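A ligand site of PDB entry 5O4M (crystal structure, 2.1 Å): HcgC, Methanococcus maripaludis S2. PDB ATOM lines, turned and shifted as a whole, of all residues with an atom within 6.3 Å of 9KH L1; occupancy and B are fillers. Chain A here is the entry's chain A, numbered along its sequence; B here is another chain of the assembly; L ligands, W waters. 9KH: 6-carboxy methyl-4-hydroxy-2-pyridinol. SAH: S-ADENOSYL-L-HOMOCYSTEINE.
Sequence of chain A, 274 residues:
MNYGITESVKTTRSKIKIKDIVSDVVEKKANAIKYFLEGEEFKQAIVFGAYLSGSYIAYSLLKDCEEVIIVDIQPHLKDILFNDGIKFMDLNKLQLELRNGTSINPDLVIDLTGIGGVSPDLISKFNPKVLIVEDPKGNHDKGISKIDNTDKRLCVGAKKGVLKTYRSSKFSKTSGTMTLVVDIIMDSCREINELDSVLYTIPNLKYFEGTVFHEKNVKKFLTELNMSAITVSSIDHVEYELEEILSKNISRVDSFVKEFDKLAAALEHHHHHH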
ATOM      1  N   TYR A  51      23.335  -0.530  -4.610  1.00  0.00           N
ATOM      2  CA  TYR A  51      23.157  -1.684  -3.725  1.00  0.00           C
ATOM      3  C   TYR A  51      21.936  -1.486  -2.812  1.00  0.00           C
ATOM      4  O   TYR A  51      21.739  -0.407  -2.351  1.00  0.00           O
ATOM      5  CB  TYR A  51      24.425  -1.922  -2.955  1.00  0.00           C
ATOM      6  CG  TYR A  51      24.376  -2.783  -1.722  1.00  0.00           C
ATOM      7  CD1 TYR A  51      23.892  -2.289  -0.519  1.00  0.00           C
ATOM      8  CD2 TYR A  51      24.893  -4.075  -1.739  1.00  0.00           C
ATOM      9  CE1 TYR A  51      23.885  -3.074   0.631  1.00  0.00           C
ATOM     10  CE2 TYR A  51      24.921  -4.857  -0.592  1.00  0.00           C
ATOM     11  CZ  TYR A  51      24.406  -4.358   0.593  1.00  0.00           C
ATOM     12  OH  TYR A  51      24.428  -5.147   1.707  1.00  0.00           O
ATOM     13  N   LEU A  52      21.191  -2.517  -2.472  1.00  0.00           N
ATOM     14  CA  LEU A  52      21.297  -3.896  -2.986  1.00  0.00           C
ATOM     15  C   LEU A  52      20.185  -4.085  -4.024  1.00  0.00           C
ATOM     16  O   LEU A  52      20.382  -4.758  -5.010  1.00  0.00           O
ATOM     17  CB  LEU A  52      21.138  -4.926  -1.848  1.00  0.00           C
ATOM     18  CG  LEU A  52      21.189  -6.425  -2.250  1.00  0.00           C
ATOM     19  CD1 LEU A  52      22.376  -6.734  -3.140  1.00  0.00           C
ATOM     20  CD2 LEU A  52      21.273  -7.329  -1.016  1.00  0.00           C
ATOM     21  N   LEU A 112      16.816   5.265  -3.311  1.00  0.00           N
ATOM     22  CA  LEU A 112      16.906   3.989  -2.608  1.00  0.00           C
ATOM     23  C   LEU A 112      18.074   3.972  -1.606  1.00  0.00           C
ATOM     24  O   LEU A 112      18.361   2.927  -1.036  1.00  0.00           O
ATOM     25  CB  LEU A 112      17.133   2.859  -3.616  1.00  0.00           C
ATOM     26  CG  LEU A 112      16.125   2.705  -4.740  1.00  0.00           C
ATOM     27  CD1 LEU A 112      16.565   1.637  -5.669  1.00  0.00           C
ATOM     28  CD2 LEU A 112      14.750   2.409  -4.224  1.00  0.00           C
ATOM     29  N   THR A 113      18.740   5.102  -1.375  1.00  0.00           N
ATOM     30  CA  THR A 113      19.885   5.175  -0.465  1.00  0.00           C
ATOM     31  C   THR A 113      19.558   4.968   1.055  1.00  0.00           C
ATOM     32  O   THR A 113      20.413   4.471   1.812  1.00  0.00           O
ATOM     33  CB  THR A 113      20.647   6.486  -0.720  1.00  0.00           C
ATOM     34  OG1 THR A 113      19.869   7.615  -0.308  1.00  0.00           O
ATOM     35  CG2 THR A 113      21.073   6.622  -2.178  1.00  0.00           C
ATOM     36  N   GLY A 114      18.358   5.332   1.475  1.00  0.00           N
ATOM     37  CA  GLY A 114      17.977   5.188   2.865  1.00  0.00           C
ATOM     38  C   GLY A 114      18.834   5.929   3.870  1.00  0.00           C
ATOM     39  O   GLY A 114      19.180   7.103   3.650  1.00  0.00           O
ATOM     40  N   ILE A 115      19.181   5.266   4.974  1.00  0.00           N
ATOM     41  CA  ILE A 115      19.962   5.813   6.092  1.00  0.00           C
ATOM     42  C   ILE A 115      21.295   6.441   5.674  1.00  0.00           C
ATOM     43  O   ILE A 115      22.132   5.790   5.046  1.00  0.00           O
ATOM     44  CB  ILE A 115      20.187   4.788   7.240  1.00  0.00           C
ATOM     45  CG1 ILE A 115      18.852   4.296   7.829  1.00  0.00           C
ATOM     46  CG2 ILE A 115      21.053   5.403   8.358  1.00  0.00           C
ATOM     47  CD1 ILE A 115      18.927   2.908   8.372  1.00  0.00           C
ATOM     48  N   GLY A 116      21.451   7.723   6.044  1.00  0.00           N
ATOM     49  CA  GLY A 116      22.651   8.489   5.754  1.00  0.00           C
ATOM     50  C   GLY A 116      22.953   8.697   4.294  1.00  0.00           C
ATOM     51  O   GLY A 116      24.083   9.055   3.957  1.00  0.00           O
ATOM     52  N   PRO A 136      13.687   3.564   4.754  1.00  0.00           N
ATOM     53  CA  PRO A 136      14.520   2.478   5.330  1.00  0.00           C
ATOM     54  C   PRO A 136      13.989   1.871   6.615  1.00  0.00           C
ATOM     55  O   PRO A 136      14.401   0.783   7.009  1.00  0.00           O
ATOM     56  CB  PRO A 136      15.865   3.166   5.574  1.00  0.00           C
ATOM     57  CG  PRO A 136      15.527   4.581   5.814  1.00  0.00           C
ATOM     58  CD  PRO A 136      14.307   4.878   4.999  1.00  0.00           C
ATOM     59  N   THR A 174      14.735  -2.811   9.662  1.00  0.00           N
ATOM     60  CA  THR A 174      14.743  -1.965   8.488  1.00  0.00           C
ATOM     61  C   THR A 174      14.005  -2.705   7.377  1.00  0.00           C
ATOM     62  O   THR A 174      13.638  -3.878   7.475  1.00  0.00           O
ATOM     63  CB  THR A 174      16.170  -1.561   8.055  1.00  0.00           C
ATOM     64  OG1 THR A 174      16.738  -2.572   7.210  1.00  0.00           O
ATOM     65  CG2 THR A 174      17.105  -1.177   9.225  1.00  0.00           C
ATOM     66  N   SER A 175      13.823  -1.972   6.281  1.00  0.00           N
ATOM     67  CA  SER A 175      13.220  -2.407   5.058  1.00  0.00           C
ATOM     68  C   SER A 175      14.314  -2.788   4.080  1.00  0.00           C
ATOM     69  O   SER A 175      13.996  -3.158   2.933  1.00  0.00           O
ATOM     70  CB  SER A 175      12.401  -1.285   4.460  1.00  0.00           C
ATOM     71  OG  SER A 175      13.251  -0.186   4.189  1.00  0.00           O
ATOM     72  N   GLY A 176      15.569  -2.717   4.508  1.00  0.00           N
ATOM     73  CA  GLY A 176      16.660  -3.051   3.618  1.00  0.00           C
ATOM     74  C   GLY A 176      16.674  -4.508   3.191  1.00  0.00           C
ATOM     75  O   GLY A 176      16.396  -5.395   3.993  1.00  0.00           O
ATOM     76  N   THR A 177      16.992  -4.758   1.916  1.00  0.00           N
ATOM     77  CA  THR A 177      17.090  -6.092   1.334  1.00  0.00           C
ATOM     78  C   THR A 177      18.014  -6.938   2.155  1.00  0.00           C
ATOM     79  O   THR A 177      17.649  -8.086   2.416  1.00  0.00           O
ATOM     80  CB  THR A 177      17.612  -5.980  -0.060  1.00  0.00           C
ATOM     81  OG1 THR A 177      16.816  -4.987  -0.630  1.00  0.00           O
ATOM     82  CG2 THR A 177      17.546  -7.307  -0.839  1.00  0.00           C
ATOM     83  N   MET A 178      19.186  -6.390   2.587  1.00  0.00           N
ATOM     84  CA  MET A 178      20.122  -7.198   3.416  1.00  0.00           C
ATOM     85  C   MET A 178      19.507  -7.626   4.753  1.00  0.00           C
ATOM     86  O   MET A 178      19.591  -8.800   5.167  1.00  0.00           O
ATOM     87  CB  MET A 178      21.435  -6.478   3.666  1.00  0.00           C
ATOM     88  CG  MET A 178      22.412  -7.300   4.532  1.00  0.00           C
ATOM     89  SD  MET A 178      22.980  -8.897   3.793  1.00  0.00           S
ATOM     90  CE  MET A 178      23.546  -8.355   2.250  1.00  0.00           C
ATOM     91  N   THR A 179      18.900  -6.661   5.436  1.00  0.00           N
ATOM     92  CA  THR A 179      18.226  -6.895   6.715  1.00  0.00           C
ATOM     93  C   THR A 179      17.132  -7.955   6.564  1.00  0.00           C
ATOM     94  O   THR A 179      17.045  -8.854   7.392  1.00  0.00           O
ATOM     95  CB  THR A 179      17.536  -5.614   7.235  1.00  0.00           C
ATOM     96  OG1 THR A 179      18.487  -4.588   7.451  1.00  0.00           O
ATOM     97  CG2 THR A 179      16.858  -5.825   8.523  1.00  0.00           C
ATOM     98  N   LEU A 180      16.299  -7.835   5.531  1.00  0.00           N
ATOM     99  CA  LEU A 180      15.208  -8.760   5.286  1.00  0.00           C
ATOM    100  C   LEU A 180      15.678 -10.167   5.013  1.00  0.00           C
ATOM    101  O   LEU A 180      15.127 -11.097   5.595  1.00  0.00           O
ATOM    102  CB  LEU A 180      14.276  -8.244   4.167  1.00  0.00           C
ATOM    103  CG  LEU A 180      13.523  -6.953   4.482  1.00  0.00           C
ATOM    104  CD1 LEU A 180      12.949  -6.307   3.244  1.00  0.00           C
ATOM    105  CD2 LEU A 180      12.442  -7.192   5.493  1.00  0.00           C
ATOM    106  N   GLU A 209      27.910  -7.178   3.339  1.00  0.00           N
ATOM    107  CA  GLU A 209      27.973  -5.744   3.103  1.00  0.00           C
ATOM    108  C   GLU A 209      29.425  -5.277   3.155  1.00  0.00           C
ATOM    109  O   GLU A 209      29.757  -4.341   2.476  1.00  0.00           O
ATOM    110  CB  GLU A 209      27.106  -5.002   4.137  1.00  0.00           C
ATOM    111  CG  GLU A 209      27.393  -3.519   4.340  1.00  0.00           C
ATOM    112  CD  GLU A 209      26.589  -3.024   5.520  1.00  0.00           C
ATOM    113  OE1 GLU A 209      25.357  -3.237   5.536  1.00  0.00           O
ATOM    114  OE2 GLU A 209      27.192  -2.400   6.411  1.00  0.00           O
ATOM    115  N   GLY B   4      29.815   1.560   8.301  1.00  0.00           N
ATOM    116  CA  GLY B   4      29.187   0.602   7.387  1.00  0.00           C
ATOM    117  C   GLY B   4      29.204   1.122   5.959  1.00  0.00           C
ATOM    118  O   GLY B   4      30.272   1.412   5.426  1.00  0.00           O
ATOM    119  N   ILE B   5      28.023   1.270   5.359  1.00  0.00           N
ATOM    120  CA  ILE B   5      27.845   1.769   3.985  1.00  0.00           C
ATOM    121  C   ILE B   5      28.192   3.296   3.933  1.00  0.00           C
ATOM    122  O   ILE B   5      28.701   3.779   2.947  1.00  0.00           O
ATOM    123  CB  ILE B   5      26.379   1.467   3.524  1.00  0.00           C
ATOM    124  CG1 ILE B   5      26.174  -0.057   3.441  1.00  0.00           C
ATOM    125  CG2 ILE B   5      26.072   2.144   2.194  1.00  0.00           C
ATOM    126  CD1 ILE B   5      24.766  -0.576   3.294  1.00  0.00           C
ATOM    127  N   THR B   6      27.879   4.022   5.009  1.00  0.00           N
ATOM    128  CA  THR B   6      28.139   5.462   5.159  1.00  0.00           C
ATOM    129  C   THR B   6      28.574   5.652   6.608  1.00  0.00           C
ATOM    130  O   THR B   6      28.519   4.696   7.405  1.00  0.00           O
ATOM    131  CB  THR B   6      26.848   6.339   4.899  1.00  0.00           C
ATOM    132  OG1 THR B   6      25.912   6.139   5.946  1.00  0.00           O
ATOM    133  CG2 THR B   6      26.218   6.123   3.542  1.00  0.00           C
ATOM    134  N   VAL B   9      26.145   4.815   9.832  1.00  0.00           N
ATOM    135  CA  VAL B   9      25.936   3.435  10.314  1.00  0.00           C
ATOM    136  C   VAL B   9      27.259   2.805  10.721  1.00  0.00           C
ATOM    137  O   VAL B   9      28.257   2.961  10.012  1.00  0.00           O
ATOM    138  CB  VAL B   9      25.177   2.578   9.260  1.00  0.00           C
ATOM    139  CG1 VAL B   9      24.853   1.167   9.764  1.00  0.00           C
ATOM    140  CG2 VAL B   9      23.852   3.279   8.851  1.00  0.00           C
ATOM    141  N   LEU B 199      20.372  -2.478  13.237  1.00  0.00           N
ATOM    142  CA  LEU B 199      19.699  -2.670  11.948  1.00  0.00           C
ATOM    143  C   LEU B 199      19.549  -4.162  11.752  1.00  0.00           C
ATOM    144  O   LEU B 199      18.430  -4.634  11.552  1.00  0.00           O
ATOM    145  CB  LEU B 199      20.472  -2.056  10.771  1.00  0.00           C
ATOM    146  CG  LEU B 199      20.376  -0.534  10.619  1.00  0.00           C
ATOM    147  CD1 LEU B 199      21.051   0.180  11.711  1.00  0.00           C
ATOM    148  CD2 LEU B 199      20.984  -0.104   9.324  1.00  0.00           C
ATOM    149  N   TYR B 200      20.675  -4.880  11.819  1.00  0.00           N
ATOM    150  CA  TYR B 200      20.701  -6.319  11.656  1.00  0.00           C
ATOM    151  C   TYR B 200      21.917  -6.933  12.350  1.00  0.00           C
ATOM    152  O   TYR B 200      22.907  -6.260  12.588  1.00  0.00           O
ATOM    153  CB  TYR B 200      20.575  -6.775  10.202  1.00  0.00           C
ATOM    154  CG  TYR B 200      21.753  -6.448   9.335  1.00  0.00           C
ATOM    155  CD1 TYR B 200      22.839  -7.315   9.236  1.00  0.00           C
ATOM    156  CD2 TYR B 200      21.763  -5.315   8.528  1.00  0.00           C
ATOM    157  CE1 TYR B 200      23.916  -7.045   8.393  1.00  0.00           C
ATOM    158  CE2 TYR B 200      22.842  -5.028   7.687  1.00  0.00           C
ATOM    159  CZ  TYR B 200      23.912  -5.899   7.629  1.00  0.00           C
ATOM    160  OH  TYR B 200      24.993  -5.663   6.822  1.00  0.00           O
ATOM    161  N   SER B 233      25.302  -4.349  12.617  1.00  0.00           N
ATOM    162  CA  SER B 233      25.190  -3.077  11.913  1.00  0.00           C
ATOM    163  C   SER B 233      24.229  -2.275  12.834  1.00  0.00           C
ATOM    164  O   SER B 233      23.130  -2.739  13.151  1.00  0.00           O
ATOM    165  CB  SER B 233      24.571  -3.267  10.524  1.00  0.00           C
ATOM    166  OG  SER B 233      24.265  -1.989   9.982  1.00  0.00           O
HETATM  167  C2  9KH L   1      20.017   1.552   4.499  1.00  0.00           C
HETATM  168  C3  9KH L   1      19.641   0.292   4.958  1.00  0.00           C
HETATM  169  C4  9KH L   1      20.589  -0.472   5.675  1.00  0.00           C
HETATM  170  C6  9KH L   1      22.194   1.289   5.460  1.00  0.00           C
HETATM  171  O1  9KH L   1      19.092   2.269   3.818  1.00  0.00           O
HETATM  172  N5  9KH L   1      21.822   0.044   5.891  1.00  0.00           N
HETATM  173  C7  9KH L   1      21.298   2.072   4.742  1.00  0.00           C
HETATM  174  O8  9KH L   1      23.458   1.738   5.720  1.00  0.00           O
HETATM  175  C9  9KH L   1      18.216  -0.149   4.638  1.00  0.00           C
HETATM  176  C10 9KH L   1      20.341  -1.876   6.192  1.00  0.00           C
HETATM  177  C12 9KH L   1      20.333  -2.834   4.997  1.00  0.00           C
HETATM  178  O13 9KH L   1      21.058  -2.627   3.977  1.00  0.00           O
HETATM  179  O14 9KH L   1      19.569  -3.832   5.052  1.00  0.00           O
HETATM  180  N   SAH L   2      17.721   0.556   0.082  1.00  0.00           N
HETATM  181  CA  SAH L   2      18.772  -0.395  -0.340  1.00  0.00           C
HETATM  182  CB  SAH L   2      19.991  -0.256   0.597  1.00  0.00           C
HETATM  183  CG  SAH L   2      20.712   1.070   0.388  1.00  0.00           C
HETATM  184  SD  SAH L   2      22.372   1.116   0.959  1.00  0.00           S
HETATM  185  C   SAH L   2      18.232  -1.782  -0.219  1.00  0.00           C
HETATM  186  O   SAH L   2      18.842  -2.679  -0.796  1.00  0.00           O
HETATM  187  OXT SAH L   2      17.198  -2.009   0.439  1.00  0.00           O
HETATM  188  C5' SAH L   2      22.935   2.691   0.394  1.00  0.00           C
HETATM  189  C4' SAH L   2      23.359   2.616  -1.098  1.00  0.00           C
HETATM  190  O4' SAH L   2      23.303   3.923  -1.664  1.00  0.00           O
HETATM  191  C3' SAH L   2      24.823   2.210  -1.225  1.00  0.00           C
HETATM  192  O3' SAH L   2      25.100   1.623  -2.537  1.00  0.00           O
HETATM  193  C2' SAH L   2      25.562   3.531  -1.040  1.00  0.00           C
HETATM  194  O2' SAH L   2      26.896   3.515  -1.599  1.00  0.00           O
HETATM  195  C1' SAH L   2      24.651   4.458  -1.827  1.00  0.00           C
HETATM  196  N9  SAH L   2      24.649   5.848  -1.340  1.00  0.00           N
HETATM  197  C8  SAH L   2      24.715   6.279  -0.056  1.00  0.00           C
HETATM  198  N7  SAH L   2      24.649   7.642  -0.044  1.00  0.00           N
HETATM  199  C5  SAH L   2      24.508   8.080  -1.340  1.00  0.00           C
HETATM  200  C6  SAH L   2      24.360   9.388  -2.062  1.00  0.00           C
HETATM  201  N6  SAH L   2      24.349  10.575  -1.407  1.00  0.00           N
HETATM  202  N1  SAH L   2      24.246   9.380  -3.411  1.00  0.00           N
HETATM  203  C2  SAH L   2      24.259   8.221  -4.108  1.00  0.00           C
HETATM  204  N3  SAH L   2      24.385   7.008  -3.515  1.00  0.00           N
HETATM  205  C4  SAH L   2      24.494   6.878  -2.173  1.00  0.00           C
HETATM  206  O   HOH W   1      16.497   2.476   2.224  1.00  0.00           O
HETATM  207  O   HOH W   2      23.738  -1.600   7.283  1.00  0.00           O
HETATM  208  O   HOH W   3      20.436  -3.827   1.564  1.00  0.00           O
HETATM  209  O   HOH W   4      24.051   4.240   5.711  1.00  0.00           O
HETATM  210  O   HOH W   5      23.552  -3.944   3.993  1.00  0.00           O
HETATM  211  O   HOH W   6      25.767   0.537   6.761  1.00  0.00           O
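O of SAH L2 lies within hydrogen-bond range of N of Leu 52 (2.9 Å).
The backbone carbonyl oxygen (O) of Thr 113 is in hydrogen-bond range of an oxygen (O1) of 9KH L1 (3.3 Å).
N of Thr 177 is in hydrogen-bond range of OXT of SAH L2, 3.1 Å away.
An oxygen (O3') of SAH L2 is in hydrogen-bond range of the backbone NH (N) of Tyr 51 (3.5 Å).
An oxygen (O) of SAH L2 sits at hydrogen-bond distance from the side-chain hydroxyl of Thr 177, at 3.1 Å.
O of Leu 112 lies within hydrogen-bond range of N of SAH L2.
The side-chain hydroxyl (OG1) of Thr 179 sits at hydrogen-bond distance from an oxygen (O14) of 9KH L1 (2.7 Å).
An oxygen (O1) of 9KH L1 sits at hydrogen-bond distance from the backbone NH of Ile 115.
N of Thr 179 sits at hydrogen-bond distance from O14 of 9KH L1, at 2.9 Å.
The backbone carbonyl oxygen of Pro 136 is in hydrogen-bond range of the backbone NH of Ser 175, 2.9 Å away.
OG1 of Thr 174 sits at hydrogen-bond distance from N of Gly 176 (2.9 Å).
The backbone carbonyl oxygen (O) of Val 9 of chain B lies within hydrogen-bond range of the backbone NH (N) of Gly 4 of chain B (2.7 Å).
The side-chain hydroxyl (OG1) of Thr 179 is in hydrogen-bond range of the side-chain hydroxyl (OG1) of Thr 174 (2.7 Å).
The backbone carbonyl oxygen (O) of Ser 233 of chain B is in hydrogen-bond range of the backbone NH (N) of Leu 199 of chain B.
Water W4 lies within hydrogen-bond range of the backbone carbonyl oxygen (O) of Ile 115 (2.6 Å), an oxygen (O8) of 9KH L1 (2.6 Å) and the side-chain hydroxyl (OG1) of Thr 6 of chain B (2.7 Å).
Water W3 lies within hydrogen-bond range of an oxygen (O13) of 9KH L1 (2.8 Å), the backbone NH (N) of Met 178 (3.0 Å) and an oxygen (O) of SAH L2 (3.1 Å).
Water W6 lies within hydrogen-bond range of N of Ile 5 of chain B (2.8 Å), O8 of 9KH L1 (2.8 Å) and OE2 of Glu 209 (3.3 Å).
Water W5 lies within hydrogen-bond range of OE1 of Glu 209 (2.5 Å), OH of Tyr 51 (2.7 Å) and O13 of 9KH L1 (2.8 Å).
Water W2 lies within hydrogen-bond range of OG of Ser 233 of chain B (2.8 Å), N5 of 9KH L1 (2.9 Å) and OE1 of Glu 209 (2.9 Å).
Water W1 lies within hydrogen-bond range of O1 of 9KH L1 (3.1 Å), N of SAH L2 (3.1 Å) and N of Gly 114 (3.5 Å).
Gly 114 touches 9KH L1 (CA to O1, 3.3 Å).
Pro 136 touches 9KH L1 (CB to O1, 3.8 Å).
Thr 174 touches 9KH L1.
Gly 176 touches 9KH L1.
Met 178 touches 9KH L1 (CB to O14, 3.5 Å).
Ile 5 of chain B touches 9KH L1.
Val 9 of chain B touches 9KH L1.
Leu 199 of chain B touches 9KH L1.
Hydrophobic or aromatic side chains that line 9KH L1: Ile 115, Pro 136, Met 178, Ile 5 of chain B, Val 9 of chain B and Leu 199 of chain B.
11 residues have an atom within 4 Å of 9KH L1: Thr 113, Gly 114, Ile 115, Pro 136, Thr 174, Gly 176, Met 178, Thr 179, Ile 5 of chain B, Val 9 of chain B and Leu 199 of chain B.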
